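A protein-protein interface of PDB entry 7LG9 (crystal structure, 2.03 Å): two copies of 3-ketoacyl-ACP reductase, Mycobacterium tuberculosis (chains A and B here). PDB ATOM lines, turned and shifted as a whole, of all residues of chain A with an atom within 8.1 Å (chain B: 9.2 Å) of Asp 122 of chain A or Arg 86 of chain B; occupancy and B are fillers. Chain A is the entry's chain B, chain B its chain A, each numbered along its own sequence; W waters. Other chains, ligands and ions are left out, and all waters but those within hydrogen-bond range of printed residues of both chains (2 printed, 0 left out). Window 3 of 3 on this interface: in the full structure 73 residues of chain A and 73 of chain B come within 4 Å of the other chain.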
ATOM      1  N   ASN A 119      -0.163  -9.852   3.085  1.00  0.00           N
ATOM      2  CA  ASN A 119      -0.224 -11.262   3.443  1.00  0.00           C
ATOM      3  C   ASN A 119      -1.186 -12.058   2.573  1.00  0.00           C
ATOM      4  O   ASN A 119      -1.338 -13.266   2.791  1.00  0.00           O
ATOM      5  CB  ASN A 119      -0.626 -11.423   4.916  1.00  0.00           C
ATOM      6  CG  ASN A 119       0.350 -10.760   5.862  1.00  0.00           C
ATOM      7  OD1 ASN A 119       1.563 -10.817   5.662  1.00  0.00           O
ATOM      8  ND2 ASN A 119      -0.175 -10.123   6.901  1.00  0.00           N
ATOM      9  N   MET A 120      -1.833 -11.424   1.599  1.00  0.00           N
ATOM     10  CA  MET A 120      -2.884 -12.071   0.825  1.00  0.00           C
ATOM     11  C   MET A 120      -2.288 -12.991  -0.233  1.00  0.00           C
ATOM     12  O   MET A 120      -1.435 -12.574  -1.023  1.00  0.00           O
ATOM     13  CB  MET A 120      -3.779 -11.016   0.175  1.00  0.00           C
ATOM     14  CG  MET A 120      -4.929 -11.588  -0.631  1.00  0.00           C
ATOM     15  SD  MET A 120      -6.168 -10.343  -1.041  1.00  0.00           S
ATOM     16  CE  MET A 120      -6.821  -9.969   0.587  1.00  0.00           C
ATOM     17  N   SER A 121      -2.737 -14.243  -0.241  1.00  0.00           N
ATOM     18  CA  SER A 121      -2.263 -15.223  -1.204  1.00  0.00           C
ATOM     19  C   SER A 121      -3.004 -15.077  -2.532  1.00  0.00           C
ATOM     20  O   SER A 121      -4.021 -14.385  -2.638  1.00  0.00           O
ATOM     21  CB  SER A 121      -2.433 -16.639  -0.653  1.00  0.00           C
ATOM     22  OG  SER A 121      -3.794 -16.926  -0.382  1.00  0.00           O
ATOM     23  N   ASP A 122      -2.473 -15.741  -3.562  1.00  0.00           N
ATOM     24  CA  ASP A 122      -3.128 -15.729  -4.866  1.00  0.00           C
ATOM     25  C   ASP A 122      -4.506 -16.377  -4.793  1.00  0.00           C
ATOM     26  O   ASP A 122      -5.463 -15.891  -5.410  1.00  0.00           O
ATOM     27  CB  ASP A 122      -2.262 -16.444  -5.903  1.00  0.00           C
ATOM     28  CG  ASP A 122      -0.962 -15.719  -6.186  1.00  0.00           C
ATOM     29  OD1 ASP A 122      -0.763 -14.610  -5.649  1.00  0.00           O
ATOM     30  OD2 ASP A 122      -0.137 -16.265  -6.950  1.00  0.00           O
ATOM     31  N   GLU A 123      -4.625 -17.479  -4.047  1.00  0.00           N
ATOM     32  CA  GLU A 123      -5.911 -18.158  -3.926  1.00  0.00           C
ATOM     33  C   GLU A 123      -6.938 -17.279  -3.224  1.00  0.00           C
ATOM     34  O   GLU A 123      -8.105 -17.231  -3.632  1.00  0.00           O
ATOM     35  CB  GLU A 123      -5.746 -19.484  -3.180  1.00  0.00           C
ATOM     36  CG  GLU A 123      -4.951 -20.544  -3.930  1.00  0.00           C
ATOM     37  CD  GLU A 123      -3.513 -20.637  -3.466  1.00  0.00           C
ATOM     38  OE1 GLU A 123      -2.827 -19.595  -3.421  1.00  0.00           O
ATOM     39  OE2 GLU A 123      -3.071 -21.758  -3.137  1.00  0.00           O
ATOM     40  N   GLU A 124      -6.525 -16.576  -2.165  1.00  0.00           N
ATOM     41  CA  GLU A 124      -7.448 -15.698  -1.452  1.00  0.00           C
ATOM     42  C   GLU A 124      -7.961 -14.579  -2.345  1.00  0.00           C
ATOM     43  O   GLU A 124      -9.111 -14.147  -2.202  1.00  0.00           O
ATOM     44  CB  GLU A 124      -6.771 -15.119  -0.208  1.00  0.00           C
ATOM     45  CG  GLU A 124      -6.662 -16.097   0.949  1.00  0.00           C
ATOM     46  CD  GLU A 124      -5.872 -15.539   2.111  1.00  0.00           C
ATOM     47  OE1 GLU A 124      -4.777 -14.986   1.873  1.00  0.00           O
ATOM     48  OE2 GLU A 124      -6.350 -15.648   3.260  1.00  0.00           O
ATOM     49  N   TRP A 125      -7.129 -14.098  -3.269  1.00  0.00           N
ATOM     50  CA  TRP A 125      -7.575 -13.095  -4.229  1.00  0.00           C
ATOM     51  C   TRP A 125      -8.431 -13.719  -5.323  1.00  0.00           C
ATOM     52  O   TRP A 125      -9.519 -13.221  -5.628  1.00  0.00           O
ATOM     53  CB  TRP A 125      -6.368 -12.378  -4.838  1.00  0.00           C
ATOM     54  CG  TRP A 125      -6.707 -11.422  -5.946  1.00  0.00           C
ATOM     55  CD1 TRP A 125      -6.805 -11.712  -7.277  1.00  0.00           C
ATOM     56  CD2 TRP A 125      -6.978 -10.022  -5.822  1.00  0.00           C
ATOM     57  NE1 TRP A 125      -7.127 -10.581  -7.986  1.00  0.00           N
ATOM     58  CE2 TRP A 125      -7.237  -9.529  -7.116  1.00  0.00           C
ATOM     59  CE3 TRP A 125      -7.029  -9.136  -4.741  1.00  0.00           C
ATOM     60  CZ2 TRP A 125      -7.542  -8.194  -7.360  1.00  0.00           C
ATOM     61  CZ3 TRP A 125      -7.330  -7.809  -4.986  1.00  0.00           C
ATOM     62  CH2 TRP A 125      -7.585  -7.352  -6.284  1.00  0.00           C
ATOM     63  N   ASP A 126      -7.953 -14.815  -5.919  1.00  0.00           N
ATOM     64  CA  ASP A 126      -8.669 -15.432  -7.031  1.00  0.00           C
ATOM     65  C   ASP A 126     -10.058 -15.899  -6.614  1.00  0.00           C
ATOM     66  O   ASP A 126     -11.009 -15.815  -7.401  1.00  0.00           O
ATOM     67  CB  ASP A 126      -7.861 -16.603  -7.591  1.00  0.00           C
ATOM     68  CG  ASP A 126      -6.602 -16.155  -8.309  1.00  0.00           C
ATOM     69  OD1 ASP A 126      -6.556 -14.989  -8.755  1.00  0.00           O
ATOM     70  OD2 ASP A 126      -5.664 -16.969  -8.435  1.00  0.00           O
ATOM     71  N   ALA A 127     -10.198 -16.388  -5.381  1.00  0.00           N
ATOM     72  CA  ALA A 127     -11.472 -16.954  -4.948  1.00  0.00           C
ATOM     73  C   ALA A 127     -12.543 -15.877  -4.820  1.00  0.00           C
ATOM     74  O   ALA A 127     -13.673 -16.052  -5.295  1.00  0.00           O
ATOM     75  CB  ALA A 127     -11.293 -17.698  -3.625  1.00  0.00           C
ATOM     76  N   VAL A 128     -12.210 -14.759  -4.174  1.00  0.00           N
ATOM     77  CA  VAL A 128     -13.182 -13.681  -4.012  1.00  0.00           C
ATOM     78  C   VAL A 128     -13.529 -13.067  -5.363  1.00  0.00           C
ATOM     79  O   VAL A 128     -14.689 -12.725  -5.625  1.00  0.00           O
ATOM     80  CB  VAL A 128     -12.651 -12.625  -3.026  1.00  0.00           C
ATOM     81  CG1 VAL A 128     -13.616 -11.445  -2.930  1.00  0.00           C
ATOM     82  CG2 VAL A 128     -12.434 -13.242  -1.657  1.00  0.00           C
ATOM     83  N   ILE A 129     -12.537 -12.927  -6.245  1.00  0.00           N
ATOM     84  CA  ILE A 129     -12.796 -12.364  -7.566  1.00  0.00           C
ATOM     85  C   ILE A 129     -13.684 -13.297  -8.384  1.00  0.00           C
ATOM     86  O   ILE A 129     -14.602 -12.849  -9.079  1.00  0.00           O
ATOM     87  CB  ILE A 129     -11.466 -12.062  -8.284  1.00  0.00           C
ATOM     88  CG1 ILE A 129     -10.703 -10.951  -7.558  1.00  0.00           C
ATOM     89  CG2 ILE A 129     -11.707 -11.678  -9.734  1.00  0.00           C
ATOM     90  CD1 ILE A 129     -11.451  -9.638  -7.486  1.00  0.00           C
ATOM     91  N   ASN A 180      -9.318  -7.777  -1.935  1.00  0.00           N
ATOM     92  CA  ASN A 180     -10.020  -8.637  -2.882  1.00  0.00           C
ATOM     93  C   ASN A 180     -11.512  -8.329  -2.907  1.00  0.00           C
ATOM     94  O   ASN A 180     -12.134  -8.315  -3.977  1.00  0.00           O
ATOM     95  CB  ASN A 180      -9.772 -10.103  -2.528  1.00  0.00           C
ATOM     96  CG  ASN A 180      -9.905 -10.376  -1.034  1.00  0.00           C
ATOM     97  OD1 ASN A 180     -10.291  -9.498  -0.261  1.00  0.00           O
ATOM     98  ND2 ASN A 180      -9.590 -11.600  -0.626  1.00  0.00           N
ATOM     99  N   GLY B  81       7.687 -12.037 -19.478  1.00  0.00           N
ATOM    100  CA  GLY B  81       6.683 -12.917 -18.911  1.00  0.00           C
ATOM    101  C   GLY B  81       5.310 -12.281 -18.923  1.00  0.00           C
ATOM    102  O   GLY B  81       5.142 -11.076 -19.104  1.00  0.00           O
ATOM    103  N   ASP B  82       4.301 -13.127 -18.727  1.00  0.00           N
ATOM    104  CA  ASP B  82       2.915 -12.690 -18.635  1.00  0.00           C
ATOM    105  C   ASP B  82       2.649 -12.152 -17.234  1.00  0.00           C
ATOM    106  O   ASP B  82       2.772 -12.887 -16.249  1.00  0.00           O
ATOM    107  CB  ASP B  82       1.984 -13.857 -18.964  1.00  0.00           C
ATOM    108  CG  ASP B  82       0.529 -13.443 -19.073  1.00  0.00           C
ATOM    109  OD1 ASP B  82       0.222 -12.245 -18.893  1.00  0.00           O
ATOM    110  OD2 ASP B  82      -0.313 -14.327 -19.341  1.00  0.00           O
ATOM    111  N   ILE B  83       2.275 -10.871 -17.148  1.00  0.00           N
ATOM    112  CA  ILE B  83       2.085 -10.234 -15.849  1.00  0.00           C
ATOM    113  C   ILE B  83       0.930 -10.858 -15.072  1.00  0.00           C
ATOM    114  O   ILE B  83       0.861 -10.708 -13.847  1.00  0.00           O
ATOM    115  CB  ILE B  83       1.883  -8.713 -16.024  1.00  0.00           C
ATOM    116  CG1 ILE B  83       2.089  -7.983 -14.694  1.00  0.00           C
ATOM    117  CG2 ILE B  83       0.505  -8.417 -16.592  1.00  0.00           C
ATOM    118  CD1 ILE B  83       3.416  -8.289 -14.034  1.00  0.00           C
ATOM    119  N   SER B  84       0.025 -11.565 -15.748  1.00  0.00           N
ATOM    120  CA  SER B  84      -1.046 -12.273 -15.056  1.00  0.00           C
ATOM    121  C   SER B  84      -0.564 -13.538 -14.362  1.00  0.00           C
ATOM    122  O   SER B  84      -1.322 -14.122 -13.580  1.00  0.00           O
ATOM    123  CB  SER B  84      -2.172 -12.621 -16.033  1.00  0.00           C
ATOM    124  OG  SER B  84      -1.719 -13.510 -17.038  1.00  0.00           O
ATOM    125  N   GLN B  85       0.666 -13.972 -14.625  1.00  0.00           N
ATOM    126  CA  GLN B  85       1.227 -15.157 -13.990  1.00  0.00           C
ATOM    127  C   GLN B  85       2.025 -14.765 -12.753  1.00  0.00           C
ATOM    128  O   GLN B  85       2.773 -13.782 -12.765  1.00  0.00           O
ATOM    129  CB  GLN B  85       2.118 -15.924 -14.970  1.00  0.00           C
ATOM    130  CG  GLN B  85       1.373 -16.482 -16.174  1.00  0.00           C
ATOM    131  CD  GLN B  85       0.361 -17.543 -15.792  1.00  0.00           C
ATOM    132  OE1 GLN B  85       0.725 -18.646 -15.384  1.00  0.00           O
ATOM    133  NE2 GLN B  85      -0.917 -17.213 -15.918  1.00  0.00           N
ATOM    134  N   ARG B  86       1.858 -15.545 -11.682  1.00  0.00           N
ATOM    135  CA  ARG B  86       2.553 -15.258 -10.432  1.00  0.00           C
ATOM    136  C   ARG B  86       4.066 -15.268 -10.620  1.00  0.00           C
ATOM    137  O   ARG B  86       4.783 -14.474  -9.998  1.00  0.00           O
ATOM    138  CB  ARG B  86       2.136 -16.270  -9.365  1.00  0.00           C
ATOM    139  CG  ARG B  86       2.948 -16.211  -8.082  1.00  0.00           C
ATOM    140  CD  ARG B  86       2.735 -14.900  -7.345  1.00  0.00           C
ATOM    141  NE  ARG B  86       3.501 -14.837  -6.102  1.00  0.00           N
ATOM    142  CZ  ARG B  86       3.095 -15.353  -4.945  1.00  0.00           C
ATOM    143  NH1 ARG B  86       3.857 -15.244  -3.864  1.00  0.00           N
ATOM    144  NH2 ARG B  86       1.929 -15.977  -4.867  1.00  0.00           N
ATOM    145  N   ALA B  87       4.569 -16.155 -11.483  1.00  0.00           N
ATOM    146  CA  ALA B  87       6.010 -16.270 -11.679  1.00  0.00           C
ATOM    147  C   ALA B  87       6.621 -14.976 -12.205  1.00  0.00           C
ATOM    148  O   ALA B  87       7.760 -14.643 -11.856  1.00  0.00           O
ATOM    149  CB  ALA B  87       6.315 -17.429 -12.629  1.00  0.00           C
ATOM    150  N   THR B  88       5.886 -14.234 -13.037  1.00  0.00           N
ATOM    151  CA  THR B  88       6.416 -12.984 -13.573  1.00  0.00           C
ATOM    152  C   THR B  88       6.567 -11.934 -12.479  1.00  0.00           C
ATOM    153  O   THR B  88       7.592 -11.246 -12.408  1.00  0.00           O
ATOM    154  CB  THR B  88       5.514 -12.467 -14.694  1.00  0.00           C
ATOM    155  OG1 THR B  88       5.481 -13.421 -15.764  1.00  0.00           O
ATOM    156  CG2 THR B  88       6.024 -11.137 -15.227  1.00  0.00           C
ATOM    157  N   ALA B  89       5.558 -11.801 -11.614  1.00  0.00           N
ATOM    158  CA  ALA B  89       5.652 -10.851 -10.509  1.00  0.00           C
ATOM    159  C   ALA B  89       6.765 -11.237  -9.544  1.00  0.00           C
ATOM    160  O   ALA B  89       7.445 -10.364  -8.991  1.00  0.00           O
ATOM    161  CB  ALA B  89       4.314 -10.759  -9.776  1.00  0.00           C
ATOM    162  N   ASP B  90       6.965 -12.539  -9.329  1.00  0.00           N
ATOM    163  CA  ASP B  90       8.064 -12.982  -8.477  1.00  0.00           C
ATOM    164  C   ASP B  90       9.411 -12.651  -9.105  1.00  0.00           C
ATOM    165  O   ASP B  90      10.353 -12.258  -8.406  1.00  0.00           O
ATOM    166  CB  ASP B  90       7.957 -14.485  -8.213  1.00  0.00           C
ATOM    167  CG  ASP B  90       6.769 -14.842  -7.345  1.00  0.00           C
ATOM    168  OD1 ASP B  90       6.124 -13.917  -6.809  1.00  0.00           O
ATOM    169  OD2 ASP B  90       6.478 -16.049  -7.200  1.00  0.00           O
ATOM    170  N   GLU B  91       9.521 -12.806 -10.426  1.00  0.00           N
ATOM    171  CA  GLU B  91      10.776 -12.507 -11.110  1.00  0.00           C
ATOM    172  C   GLU B  91      11.068 -11.012 -11.101  1.00  0.00           C
ATOM    173  O   GLU B  91      12.225 -10.603 -10.946  1.00  0.00           O
ATOM    174  CB  GLU B  91      10.726 -13.037 -12.543  1.00  0.00           C
ATOM    175  N   LEU B  92      10.034 -10.183 -11.264  1.00  0.00           N
ATOM    176  CA  LEU B  92      10.232  -8.737 -11.225  1.00  0.00           C
ATOM    177  C   LEU B  92      10.746  -8.286  -9.865  1.00  0.00           C
ATOM    178  O   LEU B  92      11.670  -7.466  -9.784  1.00  0.00           O
ATOM    179  CB  LEU B  92       8.928  -8.018 -11.567  1.00  0.00           C
ATOM    180  CG  LEU B  92       8.483  -8.093 -13.026  1.00  0.00           C
ATOM    181  CD1 LEU B  92       7.150  -7.389 -13.217  1.00  0.00           C
ATOM    182  CD2 LEU B  92       9.550  -7.487 -13.921  1.00  0.00           C
ATOM    183  N   LEU B  93      10.158  -8.804  -8.785  1.00  0.00           N
ATOM    184  CA  LEU B  93      10.635  -8.458  -7.451  1.00  0.00           C
ATOM    185  C   LEU B  93      12.054  -8.966  -7.228  1.00  0.00           C
ATOM    186  O   LEU B  93      12.868  -8.296  -6.582  1.00  0.00           O
ATOM    187  CB  LEU B  93       9.685  -9.017  -6.392  1.00  0.00           C
ATOM    188  CG  LEU B  93      10.060  -8.775  -4.928  1.00  0.00           C
ATOM    189  CD1 LEU B  93      10.267  -7.292  -4.658  1.00  0.00           C
ATOM    190  CD2 LEU B  93       9.002  -9.348  -3.999  1.00  0.00           C
ATOM    191  N   ALA B  94      12.370 -10.147  -7.764  1.00  0.00           N
ATOM    192  CA  ALA B  94      13.711 -10.701  -7.604  1.00  0.00           C
ATOM    193  C   ALA B  94      14.750  -9.840  -8.311  1.00  0.00           C
ATOM    194  O   ALA B  94      15.806  -9.532  -7.746  1.00  0.00           O
ATOM    195  CB  ALA B  94      13.750 -12.137  -8.128  1.00  0.00           C
ATOM    196  N   ALA B 130      -7.494 -10.844 -16.140  1.00  0.00           N
ATOM    197  CA  ALA B 130      -6.233 -11.439 -15.710  1.00  0.00           C
ATOM    198  C   ALA B 130      -5.077 -10.451 -15.841  1.00  0.00           C
ATOM    199  O   ALA B 130      -4.324 -10.229 -14.886  1.00  0.00           O
ATOM    200  CB  ALA B 130      -5.954 -12.705 -16.519  1.00  0.00           C
ATOM    201  N   ARG B 134      -5.655  -8.953 -12.171  1.00  0.00           N
ATOM    202  CA  ARG B 134      -4.774  -9.899 -11.494  1.00  0.00           C
ATOM    203  C   ARG B 134      -3.311  -9.509 -11.665  1.00  0.00           C
ATOM    204  O   ARG B 134      -2.510  -9.659 -10.735  1.00  0.00           O
ATOM    205  CB  ARG B 134      -5.020 -11.320 -12.007  1.00  0.00           C
ATOM    206  CG  ARG B 134      -4.333 -12.407 -11.181  1.00  0.00           C
ATOM    207  CD  ARG B 134      -4.597 -13.799 -11.737  1.00  0.00           C
ATOM    208  NE  ARG B 134      -4.342 -14.839 -10.743  1.00  0.00           N
ATOM    209  CZ  ARG B 134      -3.214 -15.534 -10.649  1.00  0.00           C
ATOM    210  NH1 ARG B 134      -3.083 -16.459  -9.708  1.00  0.00           N
ATOM    211  NH2 ARG B 134      -2.218 -15.312 -11.496  1.00  0.00           N
ATOM    212  N   GLY B 135      -2.947  -9.000 -12.842  1.00  0.00           N
ATOM    213  CA  GLY B 135      -1.589  -8.520 -13.035  1.00  0.00           C
ATOM    214  C   GLY B 135      -1.245  -7.373 -12.106  1.00  0.00           C
ATOM    215  O   GLY B 135      -0.135  -7.303 -11.573  1.00  0.00           O
ATOM    216  N   PHE B 137      -2.710  -6.937  -9.162  1.00  0.00           N
ATOM    217  CA  PHE B 137      -2.697  -7.482  -7.806  1.00  0.00           C
ATOM    218  C   PHE B 137      -1.372  -8.164  -7.491  1.00  0.00           C
ATOM    219  O   PHE B 137      -0.779  -7.931  -6.431  1.00  0.00           O
ATOM    220  CB  PHE B 137      -3.850  -8.467  -7.613  1.00  0.00           C
ATOM    221  CG  PHE B 137      -3.623  -9.433  -6.487  1.00  0.00           C
ATOM    222  CD1 PHE B 137      -3.704  -9.010  -5.171  1.00  0.00           C
ATOM    223  CD2 PHE B 137      -3.304 -10.756  -6.741  1.00  0.00           C
ATOM    224  CE1 PHE B 137      -3.486  -9.888  -4.131  1.00  0.00           C
ATOM    225  CE2 PHE B 137      -3.082 -11.640  -5.704  1.00  0.00           C
ATOM    226  CZ  PHE B 137      -3.173 -11.204  -4.395  1.00  0.00           C
ATOM    227  N   LEU B 138      -0.904  -9.027  -8.397  1.00  0.00           N
ATOM    228  CA  LEU B 138       0.303  -9.806  -8.135  1.00  0.00           C
ATOM    229  C   LEU B 138       1.497  -8.903  -7.864  1.00  0.00           C
ATOM    230  O   LEU B 138       2.260  -9.129  -6.916  1.00  0.00           O
ATOM    231  CB  LEU B 138       0.587 -10.737  -9.315  1.00  0.00           C
ATOM    232  CG  LEU B 138      -0.445 -11.835  -9.574  1.00  0.00           C
ATOM    233  CD1 LEU B 138      -0.086 -12.641 -10.814  1.00  0.00           C
ATOM    234  CD2 LEU B 138      -0.573 -12.739  -8.360  1.00  0.00           C
ATOM    235  N   LEU B 139       1.671  -7.865  -8.683  1.00  0.00           N
ATOM    236  CA  LEU B 139       2.797  -6.962  -8.476  1.00  0.00           C
ATOM    237  C   LEU B 139       2.558  -6.035  -7.289  1.00  0.00           C
ATOM    238  O   LEU B 139       3.500  -5.682  -6.571  1.00  0.00           O
ATOM    239  CB  LEU B 139       3.066  -6.158  -9.751  1.00  0.00           C
ATOM    240  CG  LEU B 139       4.444  -5.491  -9.814  1.00  0.00           C
ATOM    241  CD1 LEU B 139       5.521  -6.507  -9.483  1.00  0.00           C
ATOM    242  CD2 LEU B 139       4.697  -4.868 -11.181  1.00  0.00           C
ATOM    243  N   ARG B 141       0.691  -6.801  -4.576  1.00  0.00           N
ATOM    244  CA  ARG B 141       0.834  -7.621  -3.376  1.00  0.00           C
ATOM    245  C   ARG B 141       2.300  -7.917  -3.082  1.00  0.00           C
ATOM    246  O   ARG B 141       2.735  -7.846  -1.926  1.00  0.00           O
ATOM    247  CB  ARG B 141       0.035  -8.916  -3.536  1.00  0.00           C
ATOM    248  CG  ARG B 141      -0.149  -9.737  -2.264  1.00  0.00           C
ATOM    249  CD  ARG B 141       1.001 -10.706  -2.039  1.00  0.00           C
ATOM    250  NE  ARG B 141       1.487 -11.252  -3.301  1.00  0.00           N
ATOM    251  CZ  ARG B 141       0.962 -12.309  -3.911  1.00  0.00           C
ATOM    252  NH1 ARG B 141      -0.071 -12.942  -3.372  1.00  0.00           N
ATOM    253  NH2 ARG B 141       1.468 -12.731  -5.060  1.00  0.00           N
ATOM    254  N   ASN B 142       3.076  -8.257  -4.114  1.00  0.00           N
ATOM    255  CA  ASN B 142       4.496  -8.536  -3.915  1.00  0.00           C
ATOM    256  C   ASN B 142       5.226  -7.309  -3.383  1.00  0.00           C
ATOM    257  O   ASN B 142       6.009  -7.400  -2.431  1.00  0.00           O
ATOM    258  CB  ASN B 142       5.126  -9.015  -5.225  1.00  0.00           C
ATOM    259  CG  ASN B 142       4.758 -10.445  -5.564  1.00  0.00           C
ATOM    260  OD1 ASN B 142       3.790 -10.992  -5.038  1.00  0.00           O
ATOM    261  ND2 ASN B 142       5.533 -11.060  -6.449  1.00  0.00           N
ATOM    262  N   ALA B 143       4.972  -6.144  -3.985  1.00  0.00           N
ATOM    263  CA  ALA B 143       5.613  -4.917  -3.523  1.00  0.00           C
ATOM    264  C   ALA B 143       5.154  -4.551  -2.117  1.00  0.00           C
ATOM    265  O   ALA B 143       5.942  -4.042  -1.310  1.00  0.00           O
ATOM    266  CB  ALA B 143       5.327  -3.777  -4.500  1.00  0.00           C
ATOM    267  N   ALA B 145       4.273  -6.722   0.204  1.00  0.00           N
ATOM    268  CA  ALA B 145       4.947  -7.636   1.121  1.00  0.00           C
ATOM    269  C   ALA B 145       6.403  -7.238   1.323  1.00  0.00           C
ATOM    270  O   ALA B 145       6.917  -7.297   2.445  1.00  0.00           O
ATOM    271  CB  ALA B 145       4.846  -9.071   0.605  1.00  0.00           C
HETATM  272  O   HOH W   1      -0.353 -17.821  -3.001  1.00  0.00           O
HETATM  273  O   HOH W   2      -1.167 -18.504  -8.369  1.00  0.00           O
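NH1 of Arg 141 of chain B is in hydrogen-bond range of O of Met 120 of chain A (2.7 Å). OD2 of Asp 126 of chain A is in salt-bridge range of NH1 of Arg 134 of chain B (2.9 Å). NH2 of Arg 86 of chain B lies within salt-bridge range of OD2 of Asp 122 of chain A (2.9 Å). The side-chain carboxylate of Asp 122 of chain A lies within salt-bridge range of the guanidinium group of Arg 141 of chain B (2.9 Å).
OD1 of Asp 90 of chain B lies within salt-bridge range of NE of Arg 86 of chain B, at 2.9 Å. The side-chain sulfur (SD) of Met 120 of chain A lies close to the side-chain amide nitrogen (ND2) of Asn 180 of chain A (3.7 Å). The backbone carbonyl oxygen (O) of Leu 138 of chain B sits close to the side-chain amide oxygen (OD1) of Asn 142 of chain B, 3.1 Å away. N of Ser 121 of chain A is in hydrogen-bond range of OE1 of Glu 124 of chain A (3.0 Å). The guanidinium group (NH2) of Arg 134 of chain B lies within hydrogen-bond range of the backbone carbonyl oxygen (O) of Ser 84 of chain B, at 2.6 Å. The guanidinium group (NE) of Arg 141 of chain B lies within hydrogen-bond range of the side-chain amide oxygen (OD1) of Asn 142 of chain B, at 2.9 Å.
Among the printed residues, pairs that only touch across the chains: Ser 121 of chain A with Phe 137 of chain B (3.7 Å), Ser 121 of chain A with Arg 141 of chain B (3.7 Å), Asp 122 of chain A with Arg 134 of chain B (3.9 Å), Asp 122 of chain A with Phe 137 of chain B (3.8 Å), Asp 122 of chain A with Leu 138 of chain B (3.3 Å) and Trp 125 of chain A with Phe 137 of chain B (3.4 Å).
Of the printed residues of chain B, Met 120 of chain A touches Arg 141. Ser 121 of chain A touches two residues of chain B. Arg 86 of chain B touches one residue of chain A. No residue of chain A comes within 4 Å of Ala 87 of chain B. Printed residues of chain A within 4 Å of Arg 141 of chain B: Met 120, Ser 121 and Asp 122. The nearest residue of chain A that does not touch Arg 86 of chain B is Ser 121 of chain A (5.5 Å).
Of the 12 printed residues of chain A, 5 touch a printed residue of chain B. Printed residues of chain B that touch a printed residue of chain A: Arg 86, Arg 134, Phe 137, Leu 138 and Arg 141. Hydrophobic or aromatic side chains of chain B that line the printed part of chain A: Phe 137 and Leu 138. Among the printed residues, 10 pairs touch across the chains. Among the printed residues, Asp or Glu carboxylates within 4 Å of a Lys or Arg side-chain nitrogen of the other chain: Asp 122 of chain A with Arg 86 of chain B (2.9 Å), Asp 122 of chain A with Arg 141 of chain B (2.9 Å) and Asp 126 of chain A with Arg 134 of chain B (2.9 Å).
No position is printed for both chains. Of the 10 pairs that touch across the chains among the printed residues, none has its exchanged pair printed and touching as well.
Water W2 bridges OD2 of Asp 122 of chain A (2.8 Å) and NH1 of Arg 134 of chain B (3.1 Å). Water W1 lies within hydrogen-bond range of N of Asp 122 of chain A (3.0 Å), OE1 of Glu 123 of chain A (3.1 Å) and NH2 of Arg 86 of chain B (3.5 Å).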
